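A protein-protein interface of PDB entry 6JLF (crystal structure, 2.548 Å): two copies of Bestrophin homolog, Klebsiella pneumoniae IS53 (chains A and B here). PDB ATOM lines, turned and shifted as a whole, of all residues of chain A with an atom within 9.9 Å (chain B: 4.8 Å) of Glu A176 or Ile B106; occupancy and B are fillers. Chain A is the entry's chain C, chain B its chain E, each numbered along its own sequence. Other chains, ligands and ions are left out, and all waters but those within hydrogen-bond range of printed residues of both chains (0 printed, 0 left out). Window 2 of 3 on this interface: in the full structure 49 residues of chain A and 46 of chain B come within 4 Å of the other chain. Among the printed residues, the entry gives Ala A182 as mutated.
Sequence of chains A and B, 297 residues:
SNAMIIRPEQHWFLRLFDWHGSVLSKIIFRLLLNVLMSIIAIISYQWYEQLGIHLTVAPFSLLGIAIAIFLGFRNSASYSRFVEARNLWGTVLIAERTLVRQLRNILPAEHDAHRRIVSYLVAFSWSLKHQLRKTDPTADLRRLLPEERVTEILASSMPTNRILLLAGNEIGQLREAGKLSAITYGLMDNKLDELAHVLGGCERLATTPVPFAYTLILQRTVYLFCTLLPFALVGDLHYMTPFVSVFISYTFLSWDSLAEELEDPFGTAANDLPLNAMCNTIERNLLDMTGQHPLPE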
ATOM      1  N   LEU A 107      10.810   5.257 -29.033  1.00  0.00           N
ATOM      2  CA  LEU A 107      10.693   4.640 -30.351  1.00  0.00           C
ATOM      3  C   LEU A 107       9.237   4.699 -30.808  1.00  0.00           C
ATOM      4  O   LEU A 107       8.540   3.678 -30.832  1.00  0.00           O
ATOM      5  CB  LEU A 107      11.217   3.206 -30.299  1.00  0.00           C
ATOM      6  CG  LEU A 107      12.665   3.086 -29.775  1.00  0.00           C
ATOM      7  CD1 LEU A 107      13.167   1.653 -29.726  1.00  0.00           C
ATOM      8  CD2 LEU A 107      13.587   3.904 -30.652  1.00  0.00           C
ATOM      9  N   LEU A 165      13.077 -13.240 -19.788  1.00  0.00           N
ATOM     10  CA  LEU A 165      14.243 -13.346 -20.659  1.00  0.00           C
ATOM     11  C   LEU A 165      13.882 -12.969 -22.088  1.00  0.00           C
ATOM     12  O   LEU A 165      14.587 -12.172 -22.717  1.00  0.00           O
ATOM     13  CB  LEU A 165      14.850 -14.746 -20.594  1.00  0.00           C
ATOM     14  CG  LEU A 165      15.974 -14.890 -21.601  1.00  0.00           C
ATOM     15  CD1 LEU A 165      17.199 -14.325 -20.947  1.00  0.00           C
ATOM     16  CD2 LEU A 165      16.224 -16.339 -21.972  1.00  0.00           C
ATOM     17  N   GLY A 168      13.414  -9.416 -22.587  1.00  0.00           N
ATOM     18  CA  GLY A 168      14.723  -8.775 -22.578  1.00  0.00           C
ATOM     19  C   GLY A 168      15.454  -8.879 -23.905  1.00  0.00           C
ATOM     20  O   GLY A 168      16.087  -7.913 -24.340  1.00  0.00           O
ATOM     21  N   ASN A 169      15.378 -10.045 -24.572  1.00  0.00           N
ATOM     22  CA  ASN A 169      15.973 -10.162 -25.909  1.00  0.00           C
ATOM     23  C   ASN A 169      15.439  -9.089 -26.845  1.00  0.00           C
ATOM     24  O   ASN A 169      16.210  -8.451 -27.566  1.00  0.00           O
ATOM     25  CB  ASN A 169      15.720 -11.530 -26.526  1.00  0.00           C
ATOM     26  CG  ASN A 169      16.475 -12.647 -25.836  1.00  0.00           C
ATOM     27  OD1 ASN A 169      17.479 -12.418 -25.138  1.00  0.00           O
ATOM     28  ND2 ASN A 169      16.001 -13.886 -26.033  1.00  0.00           N
ATOM     29  N   GLU A 170      14.126  -8.850 -26.829  1.00  0.00           N
ATOM     30  CA  GLU A 170      13.562  -7.807 -27.684  1.00  0.00           C
ATOM     31  C   GLU A 170      14.203  -6.459 -27.401  1.00  0.00           C
ATOM     32  O   GLU A 170      14.617  -5.760 -28.325  1.00  0.00           O
ATOM     33  CB  GLU A 170      12.044  -7.714 -27.512  1.00  0.00           C
ATOM     34  CG  GLU A 170      11.296  -8.954 -28.000  1.00  0.00           C
ATOM     35  CD  GLU A 170      11.258  -9.109 -29.524  1.00  0.00           C
ATOM     36  OE1 GLU A 170      11.463  -8.106 -30.252  1.00  0.00           O
ATOM     37  OE2 GLU A 170      11.011 -10.244 -29.994  1.00  0.00           O
ATOM     38  N   ILE A 171      14.310  -6.077 -26.126  1.00  0.00           N
ATOM     39  CA  ILE A 171      14.959  -4.805 -25.801  1.00  0.00           C
ATOM     40  C   ILE A 171      16.436  -4.856 -26.162  1.00  0.00           C
ATOM     41  O   ILE A 171      17.033  -3.838 -26.527  1.00  0.00           O
ATOM     42  CB  ILE A 171      14.782  -4.457 -24.316  1.00  0.00           C
ATOM     43  CG1 ILE A 171      13.343  -4.689 -23.878  1.00  0.00           C
ATOM     44  CG2 ILE A 171      15.152  -3.019 -24.081  1.00  0.00           C
ATOM     45  CD1 ILE A 171      12.459  -3.594 -24.258  1.00  0.00           C
ATOM     46  N   GLY A 172      17.052  -6.033 -26.036  1.00  0.00           N
ATOM     47  CA  GLY A 172      18.438  -6.187 -26.447  1.00  0.00           C
ATOM     48  C   GLY A 172      18.645  -5.907 -27.924  1.00  0.00           C
ATOM     49  O   GLY A 172      19.544  -5.154 -28.304  1.00  0.00           O
ATOM     50  N   GLN A 173      17.816  -6.501 -28.786  1.00  0.00           N
ATOM     51  CA  GLN A 173      18.068  -6.293 -30.207  1.00  0.00           C
ATOM     52  C   GLN A 173      17.717  -4.882 -30.667  1.00  0.00           C
ATOM     53  O   GLN A 173      18.249  -4.421 -31.683  1.00  0.00           O
ATOM     54  CB  GLN A 173      17.362  -7.357 -31.060  1.00  0.00           C
ATOM     55  CG  GLN A 173      15.945  -7.730 -30.725  1.00  0.00           C
ATOM     56  CD  GLN A 173      15.685  -9.203 -31.078  1.00  0.00           C
ATOM     57  OE1 GLN A 173      16.633 -10.000 -31.135  1.00  0.00           O
ATOM     58  NE2 GLN A 173      14.409  -9.568 -31.312  1.00  0.00           N
ATOM     59  N   LEU A 174      16.889  -4.158 -29.925  1.00  0.00           N
ATOM     60  CA  LEU A 174      16.752  -2.748 -30.242  1.00  0.00           C
ATOM     61  C   LEU A 174      18.051  -2.007 -29.982  1.00  0.00           C
ATOM     62  O   LEU A 174      18.382  -1.081 -30.732  1.00  0.00           O
ATOM     63  CB  LEU A 174      15.633  -2.121 -29.434  1.00  0.00           C
ATOM     64  CG  LEU A 174      14.229  -2.594 -29.794  1.00  0.00           C
ATOM     65  CD1 LEU A 174      13.216  -1.878 -28.903  1.00  0.00           C
ATOM     66  CD2 LEU A 174      13.966  -2.299 -31.256  1.00  0.00           C
ATOM     67  N   ARG A 175      18.775  -2.394 -28.945  1.00  0.00           N
ATOM     68  CA  ARG A 175      20.087  -1.777 -28.659  1.00  0.00           C
ATOM     69  C   ARG A 175      21.123  -2.207 -29.682  1.00  0.00           C
ATOM     70  O   ARG A 175      21.836  -1.371 -30.146  1.00  0.00           O
ATOM     71  CB  ARG A 175      20.621  -2.280 -27.330  1.00  0.00           C
ATOM     72  CG  ARG A 175      21.402  -1.236 -26.561  1.00  0.00           C
ATOM     73  CD  ARG A 175      22.897  -1.351 -26.612  1.00  0.00           C
ATOM     74  NE  ARG A 175      23.366  -0.078 -27.128  1.00  0.00           N
ATOM     75  CZ  ARG A 175      24.480   0.519 -26.759  1.00  0.00           C
ATOM     76  NH1 ARG A 175      25.260  -0.050 -25.855  1.00  0.00           N
ATOM     77  NH2 ARG A 175      24.801   1.677 -27.292  1.00  0.00           N
ATOM     78  N   GLU A 176      21.203  -3.490 -29.982  1.00  0.00           N
ATOM     79  CA  GLU A 176      22.174  -3.920 -30.970  1.00  0.00           C
ATOM     80  C   GLU A 176      21.868  -3.316 -32.335  1.00  0.00           C
ATOM     81  O   GLU A 176      22.789  -3.052 -33.108  1.00  0.00           O
ATOM     82  CB  GLU A 176      22.246  -5.441 -31.054  1.00  0.00           C
ATOM     83  CG  GLU A 176      23.608  -5.956 -31.539  1.00  0.00           C
ATOM     84  CD  GLU A 176      24.549  -6.329 -30.385  1.00  0.00           C
ATOM     85  OE1 GLU A 176      25.686  -5.790 -30.351  1.00  0.00           O
ATOM     86  OE2 GLU A 176      24.167  -7.170 -29.520  1.00  0.00           O
ATOM     87  N   ALA A 177      20.605  -3.049 -32.639  1.00  0.00           N
ATOM     88  CA  ALA A 177      20.286  -2.374 -33.892  1.00  0.00           C
ATOM     89  C   ALA A 177      20.543  -0.881 -33.824  1.00  0.00           C
ATOM     90  O   ALA A 177      20.289  -0.179 -34.803  1.00  0.00           O
ATOM     91  CB  ALA A 177      18.826  -2.618 -34.285  1.00  0.00           C
ATOM     92  N   GLY A 178      21.022  -0.377 -32.694  1.00  0.00           N
ATOM     93  CA  GLY A 178      21.306   1.036 -32.578  1.00  0.00           C
ATOM     94  C   GLY A 178      20.103   1.933 -32.438  1.00  0.00           C
ATOM     95  O   GLY A 178      20.221   3.139 -32.660  1.00  0.00           O
ATOM     96  N   LYS A 179      18.940   1.405 -32.075  1.00  0.00           N
ATOM     97  CA  LYS A 179      17.796   2.294 -31.919  1.00  0.00           C
ATOM     98  C   LYS A 179      17.693   2.898 -30.521  1.00  0.00           C
ATOM     99  O   LYS A 179      16.884   3.819 -30.318  1.00  0.00           O
ATOM    100  CB  LYS A 179      16.513   1.555 -32.304  1.00  0.00           C
ATOM    101  CG  LYS A 179      16.617   0.932 -33.685  1.00  0.00           C
ATOM    102  CD  LYS A 179      15.346   0.275 -34.123  1.00  0.00           C
ATOM    103  CE  LYS A 179      15.586  -0.599 -35.345  1.00  0.00           C
ATOM    104  NZ  LYS A 179      14.315  -1.252 -35.791  1.00  0.00           N
ATOM    105  N   LEU A 180      18.515   2.435 -29.567  1.00  0.00           N
ATOM    106  CA  LEU A 180      18.539   2.955 -28.207  1.00  0.00           C
ATOM    107  C   LEU A 180      19.964   3.276 -27.800  1.00  0.00           C
ATOM    108  O   LEU A 180      20.880   2.489 -28.055  1.00  0.00           O
ATOM    109  CB  LEU A 180      17.968   1.957 -27.184  1.00  0.00           C
ATOM    110  CG  LEU A 180      16.548   1.413 -27.273  1.00  0.00           C
ATOM    111  CD1 LEU A 180      16.379   0.295 -26.254  1.00  0.00           C
ATOM    112  CD2 LEU A 180      15.549   2.513 -27.020  1.00  0.00           C
ATOM    113  N   SER A 181      20.132   4.414 -27.124  1.00  0.00           N
ATOM    114  CA  SER A 181      21.318   4.702 -26.325  1.00  0.00           C
ATOM    115  C   SER A 181      21.572   3.567 -25.344  1.00  0.00           C
ATOM    116  O   SER A 181      20.665   2.785 -25.047  1.00  0.00           O
ATOM    117  CB  SER A 181      21.152   6.000 -25.535  1.00  0.00           C
ATOM    118  OG  SER A 181      20.408   6.972 -26.254  1.00  0.00           O
ATOM    119  N   ALA A 182      22.786   3.460 -24.813  1.00  0.00           N
ATOM    120  CA  ALA A 182      22.980   2.538 -23.703  1.00  0.00           C
ATOM    121  C   ALA A 182      22.251   3.044 -22.476  1.00  0.00           C
ATOM    122  O   ALA A 182      21.671   2.258 -21.730  1.00  0.00           O
ATOM    123  CB  ALA A 182      24.466   2.345 -23.414  1.00  0.00           C
ATOM    124  N   ILE A 183      22.245   4.361 -22.276  1.00  0.00           N
ATOM    125  CA  ILE A 183      21.525   4.959 -21.158  1.00  0.00           C
ATOM    126  C   ILE A 183      20.056   4.546 -21.189  1.00  0.00           C
ATOM    127  O   ILE A 183      19.565   3.839 -20.296  1.00  0.00           O
ATOM    128  CB  ILE A 183      21.673   6.492 -21.177  1.00  0.00           C
ATOM    129  CG1 ILE A 183      23.156   6.926 -21.065  1.00  0.00           C
ATOM    130  CG2 ILE A 183      20.849   7.099 -20.058  1.00  0.00           C
ATOM    131  CD1 ILE A 183      23.891   7.147 -22.443  1.00  0.00           C
ATOM    132  N   THR A 184      19.334   4.959 -22.231  1.00  0.00           N
ATOM    133  CA  THR A 184      17.907   4.657 -22.281  1.00  0.00           C
ATOM    134  C   THR A 184      17.646   3.160 -22.435  1.00  0.00           C
ATOM    135  O   THR A 184      16.604   2.670 -22.006  1.00  0.00           O
ATOM    136  CB  THR A 184      17.231   5.444 -23.407  1.00  0.00           C
ATOM    137  OG1 THR A 184      17.538   4.823 -24.659  1.00  0.00           O
ATOM    138  CG2 THR A 184      17.702   6.905 -23.428  1.00  0.00           C
ATOM    139  N   TYR A 185      18.570   2.405 -23.020  1.00  0.00           N
ATOM    140  CA  TYR A 185      18.471   0.957 -22.886  1.00  0.00           C
ATOM    141  C   TYR A 185      18.549   0.544 -21.417  1.00  0.00           C
ATOM    142  O   TYR A 185      17.823  -0.342 -20.973  1.00  0.00           O
ATOM    143  CB  TYR A 185      19.570   0.271 -23.696  1.00  0.00           C
ATOM    144  CG  TYR A 185      19.688  -1.186 -23.412  1.00  0.00           C
ATOM    145  CD1 TYR A 185      18.744  -2.085 -23.896  1.00  0.00           C
ATOM    146  CD2 TYR A 185      20.719  -1.673 -22.638  1.00  0.00           C
ATOM    147  CE1 TYR A 185      18.839  -3.431 -23.627  1.00  0.00           C
ATOM    148  CE2 TYR A 185      20.828  -3.017 -22.358  1.00  0.00           C
ATOM    149  CZ  TYR A 185      19.886  -3.891 -22.849  1.00  0.00           C
ATOM    150  OH  TYR A 185      20.007  -5.232 -22.571  1.00  0.00           O
ATOM    151  N   GLY A 186      19.398   1.201 -20.632  1.00  0.00           N
ATOM    152  CA  GLY A 186      19.432   0.902 -19.219  1.00  0.00           C
ATOM    153  C   GLY A 186      18.179   1.317 -18.476  1.00  0.00           C
ATOM    154  O   GLY A 186      17.810   0.680 -17.489  1.00  0.00           O
ATOM    155  N   ASP A 189      15.847  -1.573 -19.118  1.00  0.00           N
ATOM    156  CA  ASP A 189      16.289  -2.778 -18.428  1.00  0.00           C
ATOM    157  C   ASP A 189      15.949  -2.706 -16.941  1.00  0.00           C
ATOM    158  O   ASP A 189      15.620  -3.727 -16.334  1.00  0.00           O
ATOM    159  CB  ASP A 189      17.782  -3.004 -18.629  1.00  0.00           C
ATOM    160  CG  ASP A 189      18.275  -4.271 -17.929  1.00  0.00           C
ATOM    161  OD1 ASP A 189      18.150  -5.337 -18.577  1.00  0.00           O
ATOM    162  OD2 ASP A 189      18.747  -4.211 -16.736  1.00  0.00           O
ATOM    163  N   LEU A 192      12.490  -4.249 -16.362  1.00  0.00           N
ATOM    164  CA  LEU A 192      12.522  -5.710 -16.279  1.00  0.00           C
ATOM    165  C   LEU A 192      13.028  -6.179 -14.922  1.00  0.00           C
ATOM    166  O   LEU A 192      12.568  -7.201 -14.418  1.00  0.00           O
ATOM    167  CB  LEU A 192      13.387  -6.294 -17.400  1.00  0.00           C
ATOM    168  CG  LEU A 192      12.949  -6.042 -18.863  1.00  0.00           C
ATOM    169  CD1 LEU A 192      13.721  -6.938 -19.806  1.00  0.00           C
ATOM    170  CD2 LEU A 192      11.447  -6.227 -19.095  1.00  0.00           C
ATOM    171  N   GLN B 102      20.761 -10.102 -18.240  1.00  0.00           N
ATOM    172  CA  GLN B 102      21.395  -9.012 -18.979  1.00  0.00           C
ATOM    173  C   GLN B 102      22.493  -9.524 -19.891  1.00  0.00           C
ATOM    174  O   GLN B 102      22.590  -9.104 -21.047  1.00  0.00           O
ATOM    175  CB  GLN B 102      21.982  -7.985 -18.021  1.00  0.00           C
ATOM    176  CG  GLN B 102      21.019  -6.958 -17.545  1.00  0.00           C
ATOM    177  CD  GLN B 102      21.679  -6.008 -16.574  1.00  0.00           C
ATOM    178  OE1 GLN B 102      21.821  -6.312 -15.367  1.00  0.00           O
ATOM    179  NE2 GLN B 102      22.088  -4.841 -17.087  1.00  0.00           N
ATOM    180  N   LEU B 103      23.348 -10.418 -19.383  1.00  0.00           N
ATOM    181  CA  LEU B 103      24.429 -10.936 -20.213  1.00  0.00           C
ATOM    182  C   LEU B 103      23.891 -11.635 -21.452  1.00  0.00           C
ATOM    183  O   LEU B 103      24.407 -11.445 -22.552  1.00  0.00           O
ATOM    184  CB  LEU B 103      25.296 -11.904 -19.412  1.00  0.00           C
ATOM    185  CG  LEU B 103      26.419 -11.294 -18.606  1.00  0.00           C
ATOM    186  CD1 LEU B 103      26.846 -12.315 -17.611  1.00  0.00           C
ATOM    187  CD2 LEU B 103      27.551 -10.940 -19.520  1.00  0.00           C
ATOM    188  N   ARG B 104      22.853 -12.454 -21.260  1.00  0.00           N
ATOM    189  CA  ARG B 104      22.220 -13.202 -22.378  1.00  0.00           C
ATOM    190  C   ARG B 104      21.605 -12.218 -23.380  1.00  0.00           C
ATOM    191  O   ARG B 104      21.704 -12.474 -24.597  1.00  0.00           O
ATOM    192  CB  ARG B 104      21.162 -14.169 -21.840  1.00  0.00           C
ATOM    193  CG  ARG B 104      20.273 -14.780 -22.914  1.00  0.00           C
ATOM    194  CD  ARG B 104      20.428 -16.287 -23.005  1.00  0.00           C
ATOM    195  NE  ARG B 104      19.837 -16.833 -24.218  1.00  0.00           N
ATOM    196  CZ  ARG B 104      19.300 -18.044 -24.314  1.00  0.00           C
ATOM    197  NH1 ARG B 104      18.786 -18.451 -25.462  1.00  0.00           N
ATOM    198  NH2 ARG B 104      19.278 -18.843 -23.262  1.00  0.00           N
ATOM    199  N   ASN B 105      20.995 -11.138 -22.879  1.00  0.00           N
ATOM    200  CA  ASN B 105      20.324 -10.153 -23.727  1.00  0.00           C
ATOM    201  C   ASN B 105      21.290  -9.187 -24.424  1.00  0.00           C
ATOM    202  O   ASN B 105      20.935  -8.649 -25.477  1.00  0.00           O
ATOM    203  CB  ASN B 105      19.328  -9.316 -22.920  1.00  0.00           C
ATOM    204  CG  ASN B 105      18.131 -10.121 -22.376  1.00  0.00           C
ATOM    205  OD1 ASN B 105      17.530  -9.733 -21.363  1.00  0.00           O
ATOM    206  ND2 ASN B 105      17.772 -11.207 -23.041  1.00  0.00           N
ATOM    207  N   ILE B 106      22.481  -8.949 -23.868  1.00  0.00           N
ATOM    208  CA  ILE B 106      23.422  -7.955 -24.390  1.00  0.00           C
ATOM    209  C   ILE B 106      24.555  -8.600 -25.178  1.00  0.00           C
ATOM    210  O   ILE B 106      24.936  -8.101 -26.234  1.00  0.00           O
ATOM    211  CB  ILE B 106      23.988  -7.067 -23.259  1.00  0.00           C
ATOM    212  CG1 ILE B 106      23.046  -5.914 -22.995  1.00  0.00           C
ATOM    213  CG2 ILE B 106      25.287  -6.443 -23.660  1.00  0.00           C
ATOM    214  CD1 ILE B 106      22.985  -4.924 -24.171  1.00  0.00           C
ATOM    215  N   LEU B 107      25.110  -9.694 -24.680  1.00  0.00           N
ATOM    216  CA  LEU B 107      26.118 -10.483 -25.374  1.00  0.00           C
ATOM    217  C   LEU B 107      25.564 -11.891 -25.560  1.00  0.00           C
ATOM    218  O   LEU B 107      26.021 -12.842 -24.916  1.00  0.00           O
ATOM    219  CB  LEU B 107      27.430 -10.515 -24.592  1.00  0.00           C
ATOM    220  CG  LEU B 107      27.856  -9.180 -24.010  1.00  0.00           C
ATOM    221  CD1 LEU B 107      29.138  -9.293 -23.217  1.00  0.00           C
ATOM    222  CD2 LEU B 107      28.030  -8.236 -25.166  1.00  0.00           C
ATOM    223  N   PRO B 108      24.557 -12.059 -26.413  1.00  0.00           N
ATOM    224  CA  PRO B 108      24.035 -13.413 -26.638  1.00  0.00           C
ATOM    225  C   PRO B 108      25.052 -14.313 -27.278  1.00  0.00           C
ATOM    226  O   PRO B 108      24.911 -15.541 -27.189  1.00  0.00           O
ATOM    227  CB  PRO B 108      22.822 -13.181 -27.548  1.00  0.00           C
ATOM    228  CG  PRO B 108      23.120 -11.901 -28.229  1.00  0.00           C
ATOM    229  CD  PRO B 108      23.843 -11.055 -27.224  1.00  0.00           C
ATOM    230  N   LYS B 179      33.421  -5.142 -24.901  1.00  0.00           N
ATOM    231  CA  LYS B 179      32.170  -5.798 -25.260  1.00  0.00           C
ATOM    232  C   LYS B 179      30.973  -5.270 -24.468  1.00  0.00           C
ATOM    233  O   LYS B 179      29.825  -5.558 -24.847  1.00  0.00           O
ATOM    234  CB  LYS B 179      32.321  -7.318 -25.106  1.00  0.00           C
ATOM    235  CG  LYS B 179      33.630  -7.843 -25.716  1.00  0.00           C
ATOM    236  CD  LYS B 179      33.789  -9.353 -25.660  1.00  0.00           C
ATOM    237  CE  LYS B 179      32.563 -10.071 -26.208  1.00  0.00           C
ATOM    238  NZ  LYS B 179      32.907 -11.417 -26.741  1.00  0.00           N
ATOM    239  N   LEU B 180      31.214  -4.485 -23.404  1.00  0.00           N
ATOM    240  CA  LEU B 180      30.170  -3.778 -22.669  1.00  0.00           C
ATOM    241  C   LEU B 180      30.500  -2.295 -22.635  1.00  0.00           C
ATOM    242  O   LEU B 180      31.667  -1.912 -22.563  1.00  0.00           O
ATOM    243  CB  LEU B 180      30.023  -4.266 -21.215  1.00  0.00           C
ATOM    244  CG  LEU B 180      29.642  -5.704 -20.930  1.00  0.00           C
ATOM    245  CD1 LEU B 180      29.850  -5.975 -19.453  1.00  0.00           C
ATOM    246  CD2 LEU B 180      28.204  -5.932 -21.344  1.00  0.00           C
ATOM    247  N   MET B 188      25.361  -3.870 -14.486  1.00  0.00           N
ATOM    248  CA  MET B 188      25.658  -5.204 -13.958  1.00  0.00           C
ATOM    249  C   MET B 188      26.404  -5.133 -12.628  1.00  0.00           C
ATOM    250  O   MET B 188      26.184  -5.962 -11.733  1.00  0.00           O
ATOM    251  CB  MET B 188      26.472  -5.995 -14.966  1.00  0.00           C
ATOM    252  CG  MET B 188      25.824  -6.036 -16.322  1.00  0.00           C
ATOM    253  SD  MET B 188      26.701  -7.158 -17.386  1.00  0.00           S
ATOM    254  CE  MET B 188      25.679  -7.044 -18.868  1.00  0.00           C
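The side-chain carboxylate (OD2) of Asp A189 is in hydrogen-bond range of the side-chain amide nitrogen (NE2) of Gln B102 (3.4 Å). ND2 of Asn B105 lies within hydrogen-bond range of OD1 of Asn A169 (2.4 Å). ND2 of Asn B105 is in hydrogen-bond range of O of Leu A165 (3.3 Å).
Among the printed residues, pairs that only touch across the chains: Tyr A185 with Ile B106 (3.1 Å), Gly A168 with Asn B105 (3.2 Å), Glu A176 with Ile B106 (3.5 Å), Gly A172 with Asn B105 (3.6 Å) and Leu A165 with Arg B104 (3.7 Å).
Gln A173 touches none of the printed residues of chain B. Leu A174 touches none of the printed residues of chain B. Of chain B, only Ile B106 (3.5 Å) comes within 4 Å of Glu A176. Of the printed residues of chain B, Asp A189 touches Gln B102. Of the printed residues of chain A, Gln B102 touches Asp A189. Ile B106 touches two residues of chain A. The nearest residue of chain B that does not touch Glu A176 is Pro B108 (4.5 Å). The nearest printed residue of chain B that does not touch Gly A172 is Ile B106 (5.2 Å).
Hydrophobic or aromatic side chains of chain B within 4 Å of the printed part of chain A: Ile B106. Hydrophobic or aromatic side chains of chain A within 4 Å of the printed part of chain B: Leu A165 and Tyr A185. Among the printed residues, 8 pairs touch across the chains.
Positions printed for both chains: 107, 179 and 180.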
